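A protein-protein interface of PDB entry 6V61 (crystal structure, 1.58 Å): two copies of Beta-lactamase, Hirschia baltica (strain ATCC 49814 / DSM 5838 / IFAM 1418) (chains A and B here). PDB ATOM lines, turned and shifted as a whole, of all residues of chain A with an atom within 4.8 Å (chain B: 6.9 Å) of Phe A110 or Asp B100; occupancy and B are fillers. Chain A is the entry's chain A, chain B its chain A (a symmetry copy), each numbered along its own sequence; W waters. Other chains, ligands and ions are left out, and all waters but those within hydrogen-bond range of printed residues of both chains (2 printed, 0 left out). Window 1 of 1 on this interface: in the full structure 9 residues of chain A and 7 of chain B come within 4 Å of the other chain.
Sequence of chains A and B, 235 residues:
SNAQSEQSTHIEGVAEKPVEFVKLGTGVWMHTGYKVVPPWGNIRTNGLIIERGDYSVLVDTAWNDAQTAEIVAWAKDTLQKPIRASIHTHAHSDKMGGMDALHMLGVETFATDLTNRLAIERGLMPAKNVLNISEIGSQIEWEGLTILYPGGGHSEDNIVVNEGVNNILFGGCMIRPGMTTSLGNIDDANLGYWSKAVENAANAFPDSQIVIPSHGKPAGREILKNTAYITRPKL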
ATOM      1  N   ALA A  85     -26.817 -18.357  26.322  1.00  0.00           N
ATOM      2  CA  ALA A  85     -25.820 -17.665  25.522  1.00  0.00           C
ATOM      3  C   ALA A  85     -26.324 -17.568  24.093  1.00  0.00           C
ATOM      4  O   ALA A  85     -27.228 -18.303  23.694  1.00  0.00           O
ATOM      5  CB  ALA A  85     -24.481 -18.390  25.562  1.00  0.00           C
ATOM      6  N   SER A  86     -25.713 -16.670  23.320  1.00  0.00           N
ATOM      7  CA  SER A  86     -26.203 -16.438  21.963  1.00  0.00           C
ATOM      8  C   SER A  86     -25.034 -16.111  21.054  1.00  0.00           C
ATOM      9  O   SER A  86     -23.979 -15.658  21.519  1.00  0.00           O
ATOM     10  CB  SER A  86     -27.210 -15.284  21.910  1.00  0.00           C
ATOM     11  OG  SER A  86     -26.583 -14.055  22.299  1.00  0.00           O
ATOM     12  N   ILE A  87     -25.226 -16.360  19.749  1.00  0.00           N
ATOM     13  CA  ILE A  87     -24.283 -15.913  18.722  1.00  0.00           C
ATOM     14  C   ILE A  87     -25.044 -15.087  17.694  1.00  0.00           C
ATOM     15  O   ILE A  87     -26.246 -15.276  17.492  1.00  0.00           O
ATOM     16  CB  ILE A  87     -23.555 -17.093  18.032  1.00  0.00           C
ATOM     17  CG1 ILE A  87     -24.553 -18.094  17.466  1.00  0.00           C
ATOM     18  CG2 ILE A  87     -22.522 -17.735  18.968  1.00  0.00           C
ATOM     19  CD1 ILE A  87     -23.874 -19.300  16.885  1.00  0.00           C
ATOM     20  N   HIS A  88     -24.341 -14.132  17.061  1.00  0.00           N
ATOM     21  CA  HIS A  88     -24.970 -13.178  16.148  1.00  0.00           C
ATOM     22  C   HIS A  88     -24.246 -13.203  14.816  1.00  0.00           C
ATOM     23  O   HIS A  88     -23.017 -13.097  14.778  1.00  0.00           O
ATOM     24  CB  HIS A  88     -24.981 -11.799  16.799  1.00  0.00           C
ATOM     25  CG  HIS A  88     -25.722 -11.854  18.091  1.00  0.00           C
ATOM     26  ND1 HIS A  88     -27.098 -11.758  18.139  1.00  0.00           N
ATOM     27  CD2 HIS A  88     -25.325 -12.237  19.325  1.00  0.00           C
ATOM     28  CE1 HIS A  88     -27.505 -11.997  19.375  1.00  0.00           C
ATOM     29  NE2 HIS A  88     -26.452 -12.305  20.108  1.00  0.00           N
ATOM     30  N   GLU A 108     -25.587 -14.478  27.681  1.00  0.00           N
ATOM     31  CA  GLU A 108     -24.201 -14.133  27.410  1.00  0.00           C
ATOM     32  C   GLU A 108     -23.985 -14.140  25.889  1.00  0.00           C
ATOM     33  O   GLU A 108     -24.099 -15.191  25.254  1.00  0.00           O
ATOM     34  CB  GLU A 108     -23.306 -15.149  28.122  1.00  0.00           C
ATOM     35  CG  GLU A 108     -21.902 -14.753  28.265  1.00  0.00           C
ATOM     36  CD  GLU A 108     -21.733 -13.502  29.124  1.00  0.00           C
ATOM     37  OE1 GLU A 108     -22.487 -13.257  30.093  1.00  0.00           O
ATOM     38  OE2 GLU A 108     -20.810 -12.775  28.814  1.00  0.00           O
ATOM     39  N   THR A 109     -23.672 -12.976  25.305  1.00  0.00           N
ATOM     40  CA  THR A 109     -23.743 -12.794  23.860  1.00  0.00           C
ATOM     41  C   THR A 109     -22.356 -12.872  23.230  1.00  0.00           C
ATOM     42  O   THR A 109     -21.378 -12.393  23.815  1.00  0.00           O
ATOM     43  CB  THR A 109     -24.378 -11.439  23.522  1.00  0.00           C
ATOM     44  OG1 THR A 109     -23.660 -10.400  24.186  1.00  0.00           O
ATOM     45  CG2 THR A 109     -25.843 -11.416  23.962  1.00  0.00           C
ATOM     46  N   PHE A 110     -22.297 -13.450  22.020  1.00  0.00           N
ATOM     47  CA  PHE A 110     -21.036 -13.664  21.296  1.00  0.00           C
ATOM     48  C   PHE A 110     -21.163 -13.170  19.863  1.00  0.00           C
ATOM     49  O   PHE A 110     -22.184 -13.398  19.200  1.00  0.00           O
ATOM     50  CB  PHE A 110     -20.644 -15.176  21.269  1.00  0.00           C
ATOM     51  CG  PHE A 110     -20.237 -15.743  22.603  1.00  0.00           C
ATOM     52  CD1 PHE A 110     -18.900 -16.045  22.859  1.00  0.00           C
ATOM     53  CD2 PHE A 110     -21.188 -15.998  23.592  1.00  0.00           C
ATOM     54  CE1 PHE A 110     -18.509 -16.574  24.081  1.00  0.00           C
ATOM     55  CE2 PHE A 110     -20.810 -16.511  24.812  1.00  0.00           C
ATOM     56  CZ  PHE A 110     -19.477 -16.807  25.064  1.00  0.00           C
ATOM     57  N   ALA A 111     -20.117 -12.515  19.374  1.00  0.00           N
ATOM     58  CA  ALA A 111     -20.021 -12.143  17.962  1.00  0.00           C
ATOM     59  C   ALA A 111     -18.542 -11.988  17.634  1.00  0.00           C
ATOM     60  O   ALA A 111     -17.695 -11.947  18.526  1.00  0.00           O
ATOM     61  CB  ALA A 111     -20.793 -10.847  17.649  1.00  0.00           C
ATOM     62  N   THR A 112     -18.235 -11.896  16.340  1.00  0.00           N
ATOM     63  CA  THR A 112     -16.844 -11.631  15.985  1.00  0.00           C
ATOM     64  C   THR A 112     -16.475 -10.179  16.306  1.00  0.00           C
ATOM     65  O   THR A 112     -17.342  -9.315  16.502  1.00  0.00           O
ATOM     66  CB  THR A 112     -16.586 -11.906  14.502  1.00  0.00           C
ATOM     67  OG1 THR A 112     -17.244 -10.908  13.713  1.00  0.00           O
ATOM     68  CG2 THR A 112     -17.056 -13.293  14.107  1.00  0.00           C
ATOM     69  N   ALA A 127     -21.954  -7.463  21.002  1.00  0.00           N
ATOM     70  CA  ALA A 127     -21.960  -8.614  21.897  1.00  0.00           C
ATOM     71  C   ALA A 127     -20.902  -8.456  22.994  1.00  0.00           C
ATOM     72  O   ALA A 127     -19.924  -7.707  22.863  1.00  0.00           O
ATOM     73  CB  ALA A 127     -21.713  -9.898  21.103  1.00  0.00           C
ATOM     74  N   ASN A 129     -18.875 -10.854  24.149  1.00  0.00           N
ATOM     75  CA  ASN A 129     -17.728 -11.739  24.004  1.00  0.00           C
ATOM     76  C   ASN A 129     -17.360 -11.847  22.535  1.00  0.00           C
ATOM     77  O   ASN A 129     -18.235 -11.859  21.668  1.00  0.00           O
ATOM     78  CB  ASN A 129     -18.047 -13.136  24.524  1.00  0.00           C
ATOM     79  CG  ASN A 129     -18.446 -13.142  25.975  1.00  0.00           C
ATOM     80  OD1 ASN A 129     -17.607 -13.241  26.845  1.00  0.00           O
ATOM     81  ND2 ASN A 129     -19.732 -13.058  26.232  1.00  0.00           N
ATOM     82  N   LEU A 131     -15.876 -13.934  19.355  1.00  0.00           N
ATOM     83  CA  LEU A 131     -15.498 -15.156  18.650  1.00  0.00           C
ATOM     84  C   LEU A 131     -14.259 -14.891  17.803  1.00  0.00           C
ATOM     85  O   LEU A 131     -14.290 -14.039  16.910  1.00  0.00           O
ATOM     86  CB  LEU A 131     -16.644 -15.599  17.741  1.00  0.00           C
ATOM     87  CG  LEU A 131     -18.025 -15.841  18.346  1.00  0.00           C
ATOM     88  CD1 LEU A 131     -19.071 -15.956  17.225  1.00  0.00           C
ATOM     89  CD2 LEU A 131     -17.996 -17.091  19.197  1.00  0.00           C
ATOM     90  N   TRP A 142     -18.515 -24.037  19.112  1.00  0.00           N
ATOM     91  CA  TRP A 142     -19.153 -23.199  20.120  1.00  0.00           C
ATOM     92  C   TRP A 142     -20.447 -23.886  20.517  1.00  0.00           C
ATOM     93  O   TRP A 142     -21.371 -23.966  19.698  1.00  0.00           O
ATOM     94  CB  TRP A 142     -19.415 -21.794  19.577  1.00  0.00           C
ATOM     95  CG  TRP A 142     -20.031 -20.820  20.568  1.00  0.00           C
ATOM     96  CD1 TRP A 142     -19.362 -20.007  21.442  1.00  0.00           C
ATOM     97  CD2 TRP A 142     -21.432 -20.555  20.771  1.00  0.00           C
ATOM     98  NE1 TRP A 142     -20.255 -19.260  22.172  1.00  0.00           N
ATOM     99  CE2 TRP A 142     -21.532 -19.568  21.774  1.00  0.00           C
ATOM    100  CE3 TRP A 142     -22.606 -21.055  20.194  1.00  0.00           C
ATOM    101  CZ2 TRP A 142     -22.761 -19.077  22.224  1.00  0.00           C
ATOM    102  CZ3 TRP A 142     -23.831 -20.565  20.639  1.00  0.00           C
ATOM    103  CH2 TRP A 142     -23.898 -19.581  21.643  1.00  0.00           C
ATOM    104  N   THR B  61      -9.202 -20.015  36.544  1.00  0.00           N
ATOM    105  CA  THR B  61      -9.808 -21.168  35.877  1.00  0.00           C
ATOM    106  C   THR B  61      -8.859 -22.355  35.975  1.00  0.00           C
ATOM    107  O   THR B  61      -7.758 -22.266  36.540  1.00  0.00           O
ATOM    108  CB  THR B  61     -10.123 -20.896  34.404  1.00  0.00           C
ATOM    109  OG1 THR B  61      -8.918 -20.899  33.622  1.00  0.00           O
ATOM    110  CG2 THR B  61     -10.843 -19.529  34.206  1.00  0.00           C
ATOM    111  N   ASP B  65     -12.351 -24.958  29.231  1.00  0.00           N
ATOM    112  CA  ASP B  65     -13.752 -24.741  29.589  1.00  0.00           C
ATOM    113  C   ASP B  65     -14.350 -25.946  30.316  1.00  0.00           C
ATOM    114  O   ASP B  65     -15.096 -25.780  31.291  1.00  0.00           O
ATOM    115  CB  ASP B  65     -14.577 -24.464  28.338  1.00  0.00           C
ATOM    116  CG  ASP B  65     -14.301 -23.110  27.715  1.00  0.00           C
ATOM    117  OD1 ASP B  65     -13.631 -22.266  28.344  1.00  0.00           O
ATOM    118  OD2 ASP B  65     -14.788 -22.907  26.574  1.00  0.00           O
ATOM    119  N   MET B  96      -6.524 -18.691  32.750  1.00  0.00           N
ATOM    120  CA  MET B  96      -7.626 -18.062  32.026  1.00  0.00           C
ATOM    121  C   MET B  96      -8.091 -18.924  30.848  1.00  0.00           C
ATOM    122  O   MET B  96      -8.814 -18.439  29.970  1.00  0.00           O
ATOM    123  CB  MET B  96      -7.219 -16.657  31.560  1.00  0.00           C
ATOM    124  CG  MET B  96      -6.945 -15.701  32.750  1.00  0.00           C
ATOM    125  SD  MET B  96      -6.368 -14.077  32.218  1.00  0.00           S
ATOM    126  CE  MET B  96      -7.949 -13.332  31.721  1.00  0.00           C
ATOM    127  N   GLY B  97      -7.692 -20.199  30.807  1.00  0.00           N
ATOM    128  CA  GLY B  97      -8.124 -21.072  29.726  1.00  0.00           C
ATOM    129  C   GLY B  97      -9.610 -21.382  29.736  1.00  0.00           C
ATOM    130  O   GLY B  97     -10.149 -21.809  28.707  1.00  0.00           O
ATOM    131  N   GLY B  98     -10.284 -21.160  30.865  1.00  0.00           N
ATOM    132  CA  GLY B  98     -11.702 -21.498  30.939  1.00  0.00           C
ATOM    133  C   GLY B  98     -12.618 -20.297  31.080  1.00  0.00           C
ATOM    134  O   GLY B  98     -13.730 -20.419  31.606  1.00  0.00           O
ATOM    135  N   MET B  99     -12.158 -19.126  30.627  1.00  0.00           N
ATOM    136  CA  MET B  99     -12.953 -17.903  30.768  1.00  0.00           C
ATOM    137  C   MET B  99     -14.317 -18.002  30.089  1.00  0.00           C
ATOM    138  O   MET B  99     -15.319 -17.503  30.630  1.00  0.00           O
ATOM    139  CB  MET B  99     -12.200 -16.700  30.189  1.00  0.00           C
ATOM    140  CG  MET B  99     -10.916 -16.377  30.906  1.00  0.00           C
ATOM    141  SD  MET B  99     -11.089 -15.928  32.646  1.00  0.00           S
ATOM    142  CE  MET B  99     -11.864 -14.324  32.529  1.00  0.00           C
ATOM    143  N   ASP B 100     -14.377 -18.574  28.882  1.00  0.00           N
ATOM    144  CA  ASP B 100     -15.661 -18.661  28.186  1.00  0.00           C
ATOM    145  C   ASP B 100     -16.667 -19.439  29.022  1.00  0.00           C
ATOM    146  O   ASP B 100     -17.846 -19.069  29.094  1.00  0.00           O
ATOM    147  CB  ASP B 100     -15.500 -19.305  26.801  1.00  0.00           C
ATOM    148  CG  ASP B 100     -14.800 -18.398  25.799  1.00  0.00           C
ATOM    149  OD1 ASP B 100     -15.242 -17.241  25.612  1.00  0.00           O
ATOM    150  OD2 ASP B 100     -13.809 -18.853  25.184  1.00  0.00           O
ATOM    151  N   ALA B 101     -16.207 -20.492  29.700  1.00  0.00           N
ATOM    152  CA  ALA B 101     -17.112 -21.263  30.552  1.00  0.00           C
ATOM    153  C   ALA B 101     -17.600 -20.427  31.725  1.00  0.00           C
ATOM    154  O   ALA B 101     -18.789 -20.467  32.070  1.00  0.00           O
ATOM    155  CB  ALA B 101     -16.412 -22.536  31.044  1.00  0.00           C
ATOM    156  N   LEU B 102     -16.699 -19.669  32.356  1.00  0.00           N
ATOM    157  CA  LEU B 102     -17.129 -18.798  33.451  1.00  0.00           C
ATOM    158  C   LEU B 102     -18.180 -17.808  32.982  1.00  0.00           C
ATOM    159  O   LEU B 102     -19.197 -17.603  33.661  1.00  0.00           O
ATOM    160  CB  LEU B 102     -15.931 -18.052  34.051  1.00  0.00           C
ATOM    161  CG  LEU B 102     -14.946 -18.922  34.818  1.00  0.00           C
ATOM    162  CD1 LEU B 102     -13.896 -17.971  35.406  1.00  0.00           C
ATOM    163  CD2 LEU B 102     -15.621 -19.731  35.898  1.00  0.00           C
ATOM    164  N   HIS B 103     -17.959 -17.189  31.818  1.00  0.00           N
ATOM    165  CA  HIS B 103     -18.904 -16.186  31.341  1.00  0.00           C
ATOM    166  C   HIS B 103     -20.248 -16.813  31.000  1.00  0.00           C
ATOM    167  O   HIS B 103     -21.293 -16.281  31.378  1.00  0.00           O
ATOM    168  CB  HIS B 103     -18.284 -15.434  30.162  1.00  0.00           C
ATOM    169  CG  HIS B 103     -17.093 -14.623  30.572  1.00  0.00           C
ATOM    170  ND1 HIS B 103     -16.107 -14.215  29.697  1.00  0.00           N
ATOM    171  CD2 HIS B 103     -16.723 -14.169  31.793  1.00  0.00           C
ATOM    172  CE1 HIS B 103     -15.188 -13.527  30.363  1.00  0.00           C
ATOM    173  NE2 HIS B 103     -15.539 -13.486  31.636  1.00  0.00           N
ATOM    174  N   MET B 104     -20.243 -17.991  30.374  1.00  0.00           N
ATOM    175  CA  MET B 104     -21.523 -18.616  30.068  1.00  0.00           C
ATOM    176  C   MET B 104     -22.254 -19.089  31.323  1.00  0.00           C
ATOM    177  O   MET B 104     -23.492 -19.181  31.315  1.00  0.00           O
ATOM    178  CB  MET B 104     -21.319 -19.763  29.087  1.00  0.00           C
ATOM    179  CG  MET B 104     -22.226 -19.570  27.879  1.00  0.00           C
ATOM    180  SD  MET B 104     -21.400 -19.911  26.343  1.00  0.00           S
ATOM    181  CE  MET B 104     -19.883 -20.642  26.915  1.00  0.00           C
ATOM    182  N   LEU B 105     -21.528 -19.380  32.393  1.00  0.00           N
ATOM    183  CA  LEU B 105     -22.118 -19.868  33.632  1.00  0.00           C
ATOM    184  C   LEU B 105     -22.450 -18.742  34.605  1.00  0.00           C
ATOM    185  O   LEU B 105     -22.777 -19.014  35.764  1.00  0.00           O
ATOM    186  CB  LEU B 105     -21.190 -20.899  34.280  1.00  0.00           C
ATOM    187  CG  LEU B 105     -21.119 -22.196  33.468  1.00  0.00           C
ATOM    188  CD1 LEU B 105     -19.887 -23.042  33.869  1.00  0.00           C
ATOM    189  CD2 LEU B 105     -22.387 -22.998  33.664  1.00  0.00           C
ATOM    190  N   GLY B 123      -4.894 -14.482  22.481  1.00  0.00           N
ATOM    191  CA  GLY B 123      -6.040 -15.278  22.101  1.00  0.00           C
ATOM    192  C   GLY B 123      -6.839 -15.806  23.267  1.00  0.00           C
ATOM    193  O   GLY B 123      -7.750 -16.622  23.062  1.00  0.00           O
ATOM    194  N   LEU B 124      -6.520 -15.381  24.486  1.00  0.00           N
ATOM    195  CA  LEU B 124      -7.329 -15.682  25.653  1.00  0.00           C
ATOM    196  C   LEU B 124      -8.431 -14.639  25.781  1.00  0.00           C
ATOM    197  O   LEU B 124      -8.345 -13.538  25.228  1.00  0.00           O
ATOM    198  CB  LEU B 124      -6.482 -15.691  26.928  1.00  0.00           C
ATOM    199  CG  LEU B 124      -5.332 -16.705  26.930  1.00  0.00           C
ATOM    200  CD1 LEU B 124      -4.329 -16.424  28.063  1.00  0.00           C
ATOM    201  CD2 LEU B 124      -5.924 -18.109  27.042  1.00  0.00           C
ATOM    202  N   MET B 125      -9.466 -15.004  26.470  1.00  0.00           N
ATOM    203  CA  MET B 125     -10.579 -14.069  26.693  1.00  0.00           C
ATOM    204  C   MET B 125     -10.308 -13.221  27.930  1.00  0.00           C
ATOM    205  O   MET B 125      -9.959 -13.767  28.970  1.00  0.00           O
ATOM    206  CB  MET B 125     -11.887 -14.828  26.884  1.00  0.00           C
ATOM    207  CG  MET B 125     -12.248 -15.733  25.715  1.00  0.00           C
ATOM    208  SD  MET B 125     -12.810 -14.805  24.270  1.00  0.00           S
ATOM    209  CE  MET B 125     -11.299 -14.587  23.351  1.00  0.00           C
HETATM  210  O   HOH W   1     -24.000 -14.774  32.024  1.00  0.00           O
HETATM  211  O   HOH W   2     -15.507 -15.004  27.023  1.00  0.00           O
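Of the printed residues of chain B, Ala A85 touches Met B104. Of the printed residues of chain B, Glu A108 touches His B103 (3.5 Å). Phe A110 touches just these residues of chain B: Asp B100 and Met B104. Printed residues of chain B within 4 Å of Asn A129: His B103 (3.4 Å). Of chain A, only Phe A110 (3.7 Å) comes within 4 Å of Asp B100. Of the printed residues of chain A, His B103 touches Glu A108 and Asn A129. Of the printed residues of chain A, Met B104 touches Ala A85 (3.4 Å) and Phe A110 (3.8 Å). The nearest printed residue of chain A that does not touch Asp B100 is Asn A129 (4.8 Å).
Water W2 lies within hydrogen-bond range of the side-chain carboxylate of Asp B100 (2.7 Å), the side-chain amide oxygen of Asn A129 (2.7 Å) and a ring nitrogen (ND1) of His B103 (2.9 Å). Water W1 lies within hydrogen-bond range of OE1 of Glu A108 (2.9 Å) and O of His B103 (3.2 Å).
OD1 of Asn A129 lies within hydrogen-bond range of ND1 of His B103 (3.4 Å). O of His B103 lies close to OE1 of Glu A108 (3.5 Å).
N of Ala A111 is in hydrogen-bond range of O of Asn A129 (3.0 Å). The side-chain carboxylate of Glu A108 is in hydrogen-bond range of the side-chain amide nitrogen of Asn A129 (2.8 Å). The backbone carbonyl oxygen of Glu A108 is in hydrogen-bond range of the backbone NH of Ser A86 (2.9 Å). The backbone NH (N) of His A88 is in hydrogen-bond range of the backbone carbonyl oxygen (O) of Phe A110. The backbone carbonyl oxygen of Ser A86 sits at hydrogen-bond distance from the backbone NH of Phe A110 (2.8 Å). The backbone carbonyl oxygen of Thr A109 sits at hydrogen-bond distance from the backbone NH of Asn A129 (3.0 Å).
Among the printed residues, merely in contact across the chains: Ala A85 with Met B104 (3.4 Å), Phe A110 with Asp B100 (3.7 Å) and Phe A110 with Met B104 (3.8 Å).
Printed residues of chain B that touch a printed residue of chain A: Asp B100, His B103 and Met B104. Of the 13 printed residues of chain A, 4 touch a printed residue of chain B. Printed residues of chain A that touch a printed residue of chain B: Ala A85, Glu A108, Phe A110 and Asn A129. Among the printed residues, 5 pairs touch across the chains.
No position is printed for both chains. Of the 5 pairs that touch across the chains among the printed residues, none has its exchanged pair printed and touching as well.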
